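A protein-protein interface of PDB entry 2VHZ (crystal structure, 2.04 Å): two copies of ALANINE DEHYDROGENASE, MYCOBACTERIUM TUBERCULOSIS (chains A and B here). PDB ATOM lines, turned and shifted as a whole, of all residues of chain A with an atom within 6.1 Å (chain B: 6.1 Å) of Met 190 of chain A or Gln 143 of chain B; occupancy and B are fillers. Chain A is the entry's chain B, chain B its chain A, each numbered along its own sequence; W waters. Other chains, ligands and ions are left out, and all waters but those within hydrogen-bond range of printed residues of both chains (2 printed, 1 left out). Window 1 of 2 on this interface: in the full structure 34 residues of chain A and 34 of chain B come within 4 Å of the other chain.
Among the printed residues, merely in contact across the chains: Gly 189 of chain A with Gly 189 of chain B, Met 150 of chain A with Leu 140 of chain B, Met 190 of chain A with Met 190 of chain B, Leu 159 of chain A with Leu 140 of chain B, Tyr 147 of chain A with Tyr 147 of chain B, Ile 186 of chain A with Met 190 of chain B, Met 190 of chain A with Gln 143 of chain B, Gln 143 of chain A with Met 190 of chain B, Leu 159 of chain A with Val 305 of chain B, Met 190 of chain A with Ile 186 of chain B, Val 158 of chain A with Val 305 of chain B, Tyr 147 of chain A with Val 144 of chain B, Tyr 147 of chain A with Gln 143 of chain B, Leu 159 of chain A with Gln 143 of chain B and Leu 159 of chain A with Arg 139 of chain B.
OE1 of Gln 143 of chain B sits close to SD of Met 150 of chain A (3.7 Å).
OH of Tyr 147 of chain B is in hydrogen-bond range of NE2 of His 148 of chain A (3.3 Å).
The side-chain amide oxygen (OE1) of Gln 143 of chain B sits close to the backbone carbonyl oxygen (O) of Ala 146 of chain A, 3.1 Å away.
O of Ala 146 of chain B lies close to OE1 of Gln 143 of chain A, 3.2 Å away.
NE2 of His 148 of chain B is in hydrogen-bond range of OH of Tyr 147 of chain A (3.3 Å).
The guanidinium group (NH1) of Arg 139 of chain B sits at hydrogen-bond distance from the backbone carbonyl oxygen (O) of Gly 162 of chain A (2.9 Å).
O of Gly 161 of chain A sits at hydrogen-bond distance from NH1 of Arg 139 of chain B (3.2 Å).
Gln 143 of chain A touches Met 190 of chain B, and with the chains exchanged Met 190 of chain A touches Gln 143 of chain B.
Tyr 147 of chain A touches Gln 143 of chain B, but with the chains exchanged Gln 143 of chain A does not touch Tyr 147 of chain B (4.04 Å).
Tyr 147 of chain B touches its own counterpart, Tyr 147 of chain A.
Ile 186 of chain A touches Met 190 of chain B, and with the chains exchanged Met 190 of chain A touches Ile 186 of chain B.
Of the 22 pairs that touch across the chains among the printed residues, 11 have their exchanged pair printed and touching as well.
Printed residues of chain B within 4 Å of Gln 143 of chain A: Ala 146 (3.2 Å) and Met 190 (3.7 Å).
Of the printed residues of chain B, Met 150 of chain A touches Leu 140 (3.5 Å) and Gln 143 (3.6 Å).
Met 190 of chain A touches just these residues of chain B: Gln 143, Ile 186 and Met 190.
The nearest printed residue of chain A that does not touch Gln 143 of chain B is Met 160 of chain A (4.1 Å).
The nearest printed residue of chain A that does not touch Arg 139 of chain B is Met 190 of chain A (5.6 Å).
Water W2 bridges the backbone carbonyl oxygen (O) of Gln 143 of chain A (2.7 Å) and the backbone carbonyl oxygen (O) of Gln 143 of chain B (2.7 Å).
Water W1 lies within hydrogen-bond range of the backbone carbonyl oxygen of Ala 146 of chain B (2.9 Å), the backbone NH of Met 160 of chain B (3.2 Å) and the side-chain amide oxygen of Gln 143 of chain A (3.3 Å).
The backbone NH (N) of Gly 161 of chain A sits close to the backbone carbonyl oxygen (O) of Met 190 of chain A (3.3 Å).
Hydrophobic or aromatic side chains of chain B within 4 Å of the printed part of chain A: Leu 140, Val 144, Ala 146, Tyr 147, His 148, Ile 186, Met 190 and Val 305.
Hydrophobic or aromatic side chains of chain A within 4 Å of the printed part of chain B: Ala 146, Tyr 147, His 148, Met 150, Leu 159, Ile 186 and Met 190.
Among the printed residues, no Asp or Glu carboxylate lies within 4 Å of a Lys or Arg side-chain nitrogen of the other chain.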
ATOM      1  N   ALA A 142      22.804 -10.677 -20.715  1.00  0.00           N
ATOM      2  CA  ALA A 142      22.985 -12.109 -20.894  1.00  0.00           C
ATOM      3  C   ALA A 142      21.773 -12.741 -21.577  1.00  0.00           C
ATOM      4  O   ALA A 142      21.919 -13.544 -22.491  1.00  0.00           O
ATOM      5  CB  ALA A 142      23.251 -12.788 -19.544  1.00  0.00           C
ATOM      6  N   GLN A 143      20.575 -12.373 -21.138  1.00  0.00           N
ATOM      7  CA  GLN A 143      19.381 -13.038 -21.641  1.00  0.00           C
ATOM      8  C   GLN A 143      19.062 -12.565 -23.056  1.00  0.00           C
ATOM      9  O   GLN A 143      18.680 -13.349 -23.916  1.00  0.00           O
ATOM     10  CB  GLN A 143      18.201 -12.863 -20.663  1.00  0.00           C
ATOM     11  CG  GLN A 143      17.284 -11.693 -20.894  1.00  0.00           C
ATOM     12  CD  GLN A 143      16.084 -11.669 -19.918  1.00  0.00           C
ATOM     13  OE1 GLN A 143      14.994 -11.168 -20.271  1.00  0.00           O
ATOM     14  NE2 GLN A 143      16.268 -12.200 -18.728  1.00  0.00           N
ATOM     15  N   ALA A 146      21.733 -14.131 -25.403  1.00  0.00           N
ATOM     16  CA  ALA A 146      21.400 -15.539 -25.680  1.00  0.00           C
ATOM     17  C   ALA A 146      20.290 -15.643 -26.716  1.00  0.00           C
ATOM     18  O   ALA A 146      20.344 -16.500 -27.621  1.00  0.00           O
ATOM     19  CB  ALA A 146      20.969 -16.259 -24.393  1.00  0.00           C
ATOM     20  N   TYR A 147      19.278 -14.781 -26.587  1.00  0.00           N
ATOM     21  CA  TYR A 147      18.155 -14.781 -27.551  1.00  0.00           C
ATOM     22  C   TYR A 147      18.614 -14.400 -28.954  1.00  0.00           C
ATOM     23  O   TYR A 147      18.174 -14.987 -29.946  1.00  0.00           O
ATOM     24  CB  TYR A 147      17.021 -13.837 -27.101  1.00  0.00           C
ATOM     25  CG  TYR A 147      15.664 -14.109 -27.754  1.00  0.00           C
ATOM     26  CD1 TYR A 147      14.835 -15.132 -27.271  1.00  0.00           C
ATOM     27  CD2 TYR A 147      15.210 -13.345 -28.830  1.00  0.00           C
ATOM     28  CE1 TYR A 147      13.586 -15.387 -27.846  1.00  0.00           C
ATOM     29  CE2 TYR A 147      13.946 -13.586 -29.416  1.00  0.00           C
ATOM     30  CZ  TYR A 147      13.161 -14.617 -28.932  1.00  0.00           C
ATOM     31  OH  TYR A 147      11.918 -14.900 -29.476  1.00  0.00           O
ATOM     32  N   HIS A 148      19.473 -13.396 -29.051  1.00  0.00           N
ATOM     33  CA  HIS A 148      19.899 -12.946 -30.369  1.00  0.00           C
ATOM     34  C   HIS A 148      20.957 -13.834 -31.030  1.00  0.00           C
ATOM     35  O   HIS A 148      21.186 -13.711 -32.243  1.00  0.00           O
ATOM     36  CB  HIS A 148      20.266 -11.451 -30.399  1.00  0.00           C
ATOM     37  CG  HIS A 148      19.075 -10.560 -30.255  1.00  0.00           C
ATOM     38  ND1 HIS A 148      18.356 -10.084 -31.337  1.00  0.00           N
ATOM     39  CD2 HIS A 148      18.412 -10.141 -29.152  1.00  0.00           C
ATOM     40  CE1 HIS A 148      17.336  -9.368 -30.900  1.00  0.00           C
ATOM     41  NE2 HIS A 148      17.352  -9.380 -29.580  1.00  0.00           N
ATOM     42  N   MET A 150      20.353 -16.880 -31.430  1.00  0.00           N
ATOM     43  CA  MET A 150      19.532 -17.829 -32.160  1.00  0.00           C
ATOM     44  C   MET A 150      19.542 -17.469 -33.639  1.00  0.00           C
ATOM     45  O   MET A 150      19.467 -16.306 -33.995  1.00  0.00           O
ATOM     46  CB  MET A 150      18.097 -17.832 -31.635  1.00  0.00           C
ATOM     47  CG  MET A 150      17.982 -18.411 -30.189  1.00  0.00           C
ATOM     48  SD  MET A 150      16.269 -18.252 -29.645  1.00  0.00           S
ATOM     49  CE  MET A 150      15.740 -19.909 -29.870  1.00  0.00           C
ATOM     50  N   VAL A 158      23.952 -20.604 -32.017  1.00  0.00           N
ATOM     51  CA  VAL A 158      24.631 -21.379 -30.973  1.00  0.00           C
ATOM     52  C   VAL A 158      23.830 -21.275 -29.661  1.00  0.00           C
ATOM     53  O   VAL A 158      23.379 -20.190 -29.289  1.00  0.00           O
ATOM     54  CB  VAL A 158      26.111 -20.901 -30.796  1.00  0.00           C
ATOM     55  CG1 VAL A 158      26.734 -21.490 -29.573  1.00  0.00           C
ATOM     56  CG2 VAL A 158      26.969 -21.357 -32.039  1.00  0.00           C
ATOM     57  N   LEU A 159      23.633 -22.405 -28.982  1.00  0.00           N
ATOM     58  CA  LEU A 159      22.944 -22.393 -27.705  1.00  0.00           C
ATOM     59  C   LEU A 159      23.916 -21.958 -26.587  1.00  0.00           C
ATOM     60  O   LEU A 159      25.048 -22.456 -26.485  1.00  0.00           O
ATOM     61  CB  LEU A 159      22.354 -23.778 -27.407  1.00  0.00           C
ATOM     62  CG  LEU A 159      21.584 -24.003 -26.104  1.00  0.00           C
ATOM     63  CD1 LEU A 159      20.262 -23.203 -26.107  1.00  0.00           C
ATOM     64  CD2 LEU A 159      21.280 -25.487 -25.918  1.00  0.00           C
ATOM     65  N   MET A 160      23.453 -21.038 -25.752  1.00  0.00           N
ATOM     66  CA  MET A 160      24.258 -20.468 -24.679  1.00  0.00           C
ATOM     67  C   MET A 160      25.118 -21.495 -23.919  1.00  0.00           C
ATOM     68  O   MET A 160      26.350 -21.363 -23.810  1.00  0.00           O
ATOM     69  CB  MET A 160      23.300 -19.734 -23.714  1.00  0.00           C
ATOM     70  CG  MET A 160      23.879 -18.563 -23.018  1.00  0.00           C
ATOM     71  SD  MET A 160      24.572 -17.223 -24.040  1.00  0.00           S
ATOM     72  CE  MET A 160      24.772 -16.162 -22.584  1.00  0.00           C
ATOM     73  N   GLY A 161      24.469 -22.523 -23.386  1.00  0.00           N
ATOM     74  CA  GLY A 161      25.164 -23.514 -22.616  1.00  0.00           C
ATOM     75  C   GLY A 161      25.565 -24.780 -23.348  1.00  0.00           C
ATOM     76  O   GLY A 161      26.064 -25.722 -22.714  1.00  0.00           O
ATOM     77  N   GLY A 162      25.353 -24.846 -24.672  1.00  0.00           N
ATOM     78  CA  GLY A 162      25.620 -26.118 -25.379  1.00  0.00           C
ATOM     79  C   GLY A 162      24.742 -27.211 -24.788  1.00  0.00           C
ATOM     80  O   GLY A 162      23.746 -26.913 -24.101  1.00  0.00           O
ATOM     81  N   ARG A 185      27.681 -13.438 -14.412  1.00  0.00           N
ATOM     82  CA  ARG A 185      27.012 -14.351 -13.540  1.00  0.00           C
ATOM     83  C   ARG A 185      25.822 -15.027 -14.257  1.00  0.00           C
ATOM     84  O   ARG A 185      25.661 -16.225 -14.185  1.00  0.00           O
ATOM     85  CB  ARG A 185      26.549 -13.597 -12.289  1.00  0.00           C
ATOM     86  CG  ARG A 185      25.502 -14.309 -11.466  1.00  0.00           C
ATOM     87  CD  ARG A 185      25.513 -13.771 -10.032  1.00  0.00           C
ATOM     88  NE  ARG A 185      24.277 -14.070  -9.311  1.00  0.00           N
ATOM     89  CZ  ARG A 185      23.897 -13.470  -8.185  1.00  0.00           C
ATOM     90  NH1 ARG A 185      22.745 -13.803  -7.630  1.00  0.00           N
ATOM     91  NH2 ARG A 185      24.639 -12.517  -7.637  1.00  0.00           N
ATOM     92  N   ILE A 186      25.003 -14.260 -14.960  1.00  0.00           N
ATOM     93  CA  ILE A 186      23.845 -14.884 -15.606  1.00  0.00           C
ATOM     94  C   ILE A 186      24.286 -15.740 -16.818  1.00  0.00           C
ATOM     95  O   ILE A 186      23.800 -16.865 -17.021  1.00  0.00           O
ATOM     96  CB  ILE A 186      22.760 -13.813 -15.998  1.00  0.00           C
ATOM     97  CG1 ILE A 186      22.257 -13.077 -14.743  1.00  0.00           C
ATOM     98  CG2 ILE A 186      21.604 -14.447 -16.807  1.00  0.00           C
ATOM     99  CD1 ILE A 186      21.896 -13.958 -13.545  1.00  0.00           C
ATOM    100  N   ALA A 187      25.218 -15.212 -17.593  1.00  0.00           N
ATOM    101  CA  ALA A 187      25.730 -15.957 -18.763  1.00  0.00           C
ATOM    102  C   ALA A 187      26.344 -17.282 -18.318  1.00  0.00           C
ATOM    103  O   ALA A 187      26.115 -18.320 -18.945  1.00  0.00           O
ATOM    104  CB  ALA A 187      26.752 -15.126 -19.530  1.00  0.00           C
ATOM    105  N   ASN A 188      27.103 -17.251 -17.225  1.00  0.00           N
ATOM    106  CA  ASN A 188      27.662 -18.469 -16.653  1.00  0.00           C
ATOM    107  C   ASN A 188      26.561 -19.428 -16.180  1.00  0.00           C
ATOM    108  O   ASN A 188      26.649 -20.647 -16.393  1.00  0.00           O
ATOM    109  CB  ASN A 188      28.632 -18.134 -15.500  1.00  0.00           C
ATOM    110  CG  ASN A 188      29.217 -19.367 -14.862  1.00  0.00           C
ATOM    111  OD1 ASN A 188      30.047 -20.036 -15.463  1.00  0.00           O
ATOM    112  ND2 ASN A 188      28.778 -19.677 -13.646  1.00  0.00           N
ATOM    113  N   GLY A 189      25.513 -18.868 -15.566  1.00  0.00           N
ATOM    114  CA  GLY A 189      24.387 -19.653 -15.074  1.00  0.00           C
ATOM    115  C   GLY A 189      23.607 -20.296 -16.213  1.00  0.00           C
ATOM    116  O   GLY A 189      22.997 -21.357 -16.042  1.00  0.00           O
ATOM    117  N   MET A 190      23.613 -19.653 -17.374  1.00  0.00           N
ATOM    118  CA  MET A 190      23.051 -20.266 -18.582  1.00  0.00           C
ATOM    119  C   MET A 190      23.996 -21.308 -19.228  1.00  0.00           C
ATOM    120  O   MET A 190      23.649 -21.899 -20.263  1.00  0.00           O
ATOM    121  CB  MET A 190      22.693 -19.187 -19.587  1.00  0.00           C
ATOM    122  CG  MET A 190      21.613 -18.221 -19.025  1.00  0.00           C
ATOM    123  SD  MET A 190      21.295 -16.859 -20.152  1.00  0.00           S
ATOM    124  CE  MET A 190      20.130 -17.679 -21.275  1.00  0.00           C
ATOM    125  N   GLY A 191      25.168 -21.520 -18.616  1.00  0.00           N
ATOM    126  CA  GLY A 191      26.123 -22.530 -19.088  1.00  0.00           C
ATOM    127  C   GLY A 191      27.150 -22.074 -20.126  1.00  0.00           C
ATOM    128  O   GLY A 191      27.943 -22.903 -20.624  1.00  0.00           O
ATOM    129  N   ALA A 192      27.161 -20.785 -20.480  1.00  0.00           N
ATOM    130  CA  ALA A 192      28.218 -20.266 -21.370  1.00  0.00           C
ATOM    131  C   ALA A 192      29.619 -20.271 -20.733  1.00  0.00           C
ATOM    132  O   ALA A 192      29.762 -20.211 -19.510  1.00  0.00           O
ATOM    133  CB  ALA A 192      27.873 -18.872 -21.835  1.00  0.00           C
ATOM    134  N   GLY B 138      14.848 -27.968 -23.621  1.00  0.00           N
ATOM    135  CA  GLY B 138      14.739 -27.556 -22.212  1.00  0.00           C
ATOM    136  C   GLY B 138      15.525 -26.287 -21.935  1.00  0.00           C
ATOM    137  O   GLY B 138      15.011 -25.328 -21.359  1.00  0.00           O
ATOM    138  N   ARG B 139      16.772 -26.262 -22.383  1.00  0.00           N
ATOM    139  CA  ARG B 139      17.591 -25.079 -22.185  1.00  0.00           C
ATOM    140  C   ARG B 139      17.001 -23.863 -22.915  1.00  0.00           C
ATOM    141  O   ARG B 139      17.007 -22.739 -22.371  1.00  0.00           O
ATOM    142  CB  ARG B 139      19.037 -25.350 -22.613  1.00  0.00           C
ATOM    143  CG  ARG B 139      19.667 -26.466 -21.759  1.00  0.00           C
ATOM    144  CD  ARG B 139      21.180 -26.595 -21.900  1.00  0.00           C
ATOM    145  NE  ARG B 139      21.578 -27.737 -21.090  1.00  0.00           N
ATOM    146  CZ  ARG B 139      22.813 -28.085 -20.772  1.00  0.00           C
ATOM    147  NH1 ARG B 139      23.839 -27.377 -21.195  1.00  0.00           N
ATOM    148  NH2 ARG B 139      23.003 -29.165 -20.009  1.00  0.00           N
ATOM    149  N   LEU B 140      16.489 -24.078 -24.130  1.00  0.00           N
ATOM    150  CA  LEU B 140      15.856 -22.976 -24.873  1.00  0.00           C
ATOM    151  C   LEU B 140      14.601 -22.440 -24.204  1.00  0.00           C
ATOM    152  O   LEU B 140      14.350 -21.245 -24.247  1.00  0.00           O
ATOM    153  CB  LEU B 140      15.512 -23.367 -26.306  1.00  0.00           C
ATOM    154  CG  LEU B 140      16.681 -23.421 -27.315  1.00  0.00           C
ATOM    155  CD1 LEU B 140      16.146 -24.102 -28.576  1.00  0.00           C
ATOM    156  CD2 LEU B 140      17.311 -22.036 -27.638  1.00  0.00           C
ATOM    157  N   ALA B 141      13.812 -23.322 -23.606  1.00  0.00           N
ATOM    158  CA  ALA B 141      12.561 -22.912 -22.944  1.00  0.00           C
ATOM    159  C   ALA B 141      12.836 -21.839 -21.869  1.00  0.00           C
ATOM    160  O   ALA B 141      12.112 -20.862 -21.741  1.00  0.00           O
ATOM    161  CB  ALA B 141      11.877 -24.143 -22.332  1.00  0.00           C
ATOM    162  N   ALA B 142      13.901 -22.041 -21.099  1.00  0.00           N
ATOM    163  CA  ALA B 142      14.278 -21.073 -20.083  1.00  0.00           C
ATOM    164  C   ALA B 142      14.638 -19.737 -20.706  1.00  0.00           C
ATOM    165  O   ALA B 142      14.167 -18.707 -20.253  1.00  0.00           O
ATOM    166  CB  ALA B 142      15.427 -21.605 -19.226  1.00  0.00           C
ATOM    167  N   GLN B 143      15.453 -19.741 -21.756  1.00  0.00           N
ATOM    168  CA  GLN B 143      15.921 -18.477 -22.319  1.00  0.00           C
ATOM    169  C   GLN B 143      14.804 -17.751 -23.085  1.00  0.00           C
ATOM    170  O   GLN B 143      14.706 -16.533 -23.054  1.00  0.00           O
ATOM    171  CB  GLN B 143      17.201 -18.682 -23.167  1.00  0.00           C
ATOM    172  CG  GLN B 143      16.999 -19.006 -24.607  1.00  0.00           C
ATOM    173  CD  GLN B 143      18.310 -19.046 -25.417  1.00  0.00           C
ATOM    174  OE1 GLN B 143      18.332 -18.638 -26.605  1.00  0.00           O
ATOM    175  NE2 GLN B 143      19.361 -19.543 -24.821  1.00  0.00           N
ATOM    176  N   VAL B 144      13.939 -18.526 -23.721  1.00  0.00           N
ATOM    177  CA  VAL B 144      12.822 -18.008 -24.483  1.00  0.00           C
ATOM    178  C   VAL B 144      11.699 -17.514 -23.516  1.00  0.00           C
ATOM    179  O   VAL B 144      11.085 -16.472 -23.755  1.00  0.00           O
ATOM    180  CB  VAL B 144      12.374 -19.140 -25.450  1.00  0.00           C
ATOM    181  CG1 VAL B 144      10.926 -19.372 -25.462  1.00  0.00           C
ATOM    182  CG2 VAL B 144      13.047 -18.980 -26.819  1.00  0.00           C
ATOM    183  N   GLY B 145      11.472 -18.246 -22.428  1.00  0.00           N
ATOM    184  CA  GLY B 145      10.567 -17.783 -21.375  1.00  0.00           C
ATOM    185  C   GLY B 145      11.001 -16.458 -20.740  1.00  0.00           C
ATOM    186  O   GLY B 145      10.184 -15.574 -20.538  1.00  0.00           O
ATOM    187  N   ALA B 146      12.302 -16.315 -20.454  1.00  0.00           N
ATOM    188  CA  ALA B 146      12.854 -15.095 -19.865  1.00  0.00           C
ATOM    189  C   ALA B 146      12.653 -13.901 -20.774  1.00  0.00           C
ATOM    190  O   ALA B 146      12.282 -12.803 -20.317  1.00  0.00           O
ATOM    191  CB  ALA B 146      14.330 -15.274 -19.593  1.00  0.00           C
ATOM    192  N   TYR B 147      12.901 -14.117 -22.065  1.00  0.00           N
ATOM    193  CA  TYR B 147      12.745 -13.062 -23.062  1.00  0.00           C
ATOM    194  C   TYR B 147      11.290 -12.639 -23.187  1.00  0.00           C
ATOM    195  O   TYR B 147      11.004 -11.454 -23.277  1.00  0.00           O
ATOM    196  CB  TYR B 147      13.301 -13.503 -24.421  1.00  0.00           C
ATOM    197  CG  TYR B 147      13.568 -12.364 -25.395  1.00  0.00           C
ATOM    198  CD1 TYR B 147      14.768 -11.644 -25.331  1.00  0.00           C
ATOM    199  CD2 TYR B 147      12.632 -12.011 -26.377  1.00  0.00           C
ATOM    200  CE1 TYR B 147      15.033 -10.607 -26.212  1.00  0.00           C
ATOM    201  CE2 TYR B 147      12.895 -10.970 -27.279  1.00  0.00           C
ATOM    202  CZ  TYR B 147      14.084 -10.277 -27.177  1.00  0.00           C
ATOM    203  OH  TYR B 147      14.385  -9.241 -28.036  1.00  0.00           O
ATOM    204  N   HIS B 148      10.372 -13.599 -23.196  1.00  0.00           N
ATOM    205  CA  HIS B 148       8.963 -13.250 -23.328  1.00  0.00           C
ATOM    206  C   HIS B 148       8.331 -12.695 -22.056  1.00  0.00           C
ATOM    207  O   HIS B 148       7.260 -12.101 -22.132  1.00  0.00           O
ATOM    208  CB  HIS B 148       8.139 -14.366 -23.980  1.00  0.00           C
ATOM    209  CG  HIS B 148       8.453 -14.530 -25.432  1.00  0.00           C
ATOM    210  ND1 HIS B 148       7.808 -13.811 -26.419  1.00  0.00           N
ATOM    211  CD2 HIS B 148       9.418 -15.242 -26.060  1.00  0.00           C
ATOM    212  CE1 HIS B 148       8.326 -14.121 -27.596  1.00  0.00           C
ATOM    213  NE2 HIS B 148       9.296 -14.994 -27.407  1.00  0.00           N
ATOM    214  N   MET B 160      14.098 -12.438 -14.788  1.00  0.00           N
ATOM    215  CA  MET B 160      14.286 -13.822 -14.317  1.00  0.00           C
ATOM    216  C   MET B 160      14.825 -13.930 -12.910  1.00  0.00           C
ATOM    217  O   MET B 160      14.218 -14.563 -12.042  1.00  0.00           O
ATOM    218  CB  MET B 160      15.210 -14.647 -15.255  1.00  0.00           C
ATOM    219  CG  MET B 160      14.500 -15.290 -16.386  1.00  0.00           C
ATOM    220  SD  MET B 160      13.186 -16.487 -16.081  1.00  0.00           S
ATOM    221  CE  MET B 160      14.055 -18.055 -16.312  1.00  0.00           C
ATOM    222  N   ILE B 186      18.681 -24.286 -16.310  1.00  0.00           N
ATOM    223  CA  ILE B 186      19.012 -22.992 -16.897  1.00  0.00           C
ATOM    224  C   ILE B 186      18.220 -21.862 -16.198  1.00  0.00           C
ATOM    225  O   ILE B 186      18.777 -20.813 -15.885  1.00  0.00           O
ATOM    226  CB  ILE B 186      18.797 -22.973 -18.446  1.00  0.00           C
ATOM    227  CG1 ILE B 186      19.696 -24.032 -19.126  1.00  0.00           C
ATOM    228  CG2 ILE B 186      19.050 -21.574 -19.010  1.00  0.00           C
ATOM    229  CD1 ILE B 186      21.170 -24.103 -18.618  1.00  0.00           C
ATOM    230  N   GLY B 189      19.887 -21.172 -13.098  1.00  0.00           N
ATOM    231  CA  GLY B 189      21.127 -20.475 -13.404  1.00  0.00           C
ATOM    232  C   GLY B 189      20.917 -18.995 -13.704  1.00  0.00           C
ATOM    233  O   GLY B 189      21.801 -18.174 -13.441  1.00  0.00           O
ATOM    234  N   MET B 190      19.754 -18.652 -14.257  1.00  0.00           N
ATOM    235  CA  MET B 190      19.392 -17.244 -14.485  1.00  0.00           C
ATOM    236  C   MET B 190      18.877 -16.548 -13.210  1.00  0.00           C
ATOM    237  O   MET B 190      18.568 -15.345 -13.234  1.00  0.00           O
ATOM    238  CB  MET B 190      18.357 -17.137 -15.598  1.00  0.00           C
ATOM    239  CG  MET B 190      18.901 -17.695 -16.939  1.00  0.00           C
ATOM    240  SD  MET B 190      17.650 -17.711 -18.233  1.00  0.00           S
ATOM    241  CE  MET B 190      17.747 -15.987 -18.816  1.00  0.00           C
ATOM    242  N   VAL B 305      19.088 -23.167 -33.014  1.00  0.00           N
ATOM    243  CA  VAL B 305      20.486 -23.260 -32.583  1.00  0.00           C
ATOM    244  C   VAL B 305      21.175 -24.449 -33.301  1.00  0.00           C
ATOM    245  O   VAL B 305      21.789 -25.315 -32.663  1.00  0.00           O
ATOM    246  CB  VAL B 305      20.627 -23.335 -31.020  1.00  0.00           C
ATOM    247  CG1 VAL B 305      20.213 -22.010 -30.343  1.00  0.00           C
ATOM    248  CG2 VAL B 305      19.825 -24.534 -30.445  1.00  0.00           C
HETATM  249  O   HOH W   1      12.995 -11.741 -17.752  1.00  0.00           O
HETATM  250  O   HOH W   2      17.076 -15.253 -22.900  1.00  0.00           O
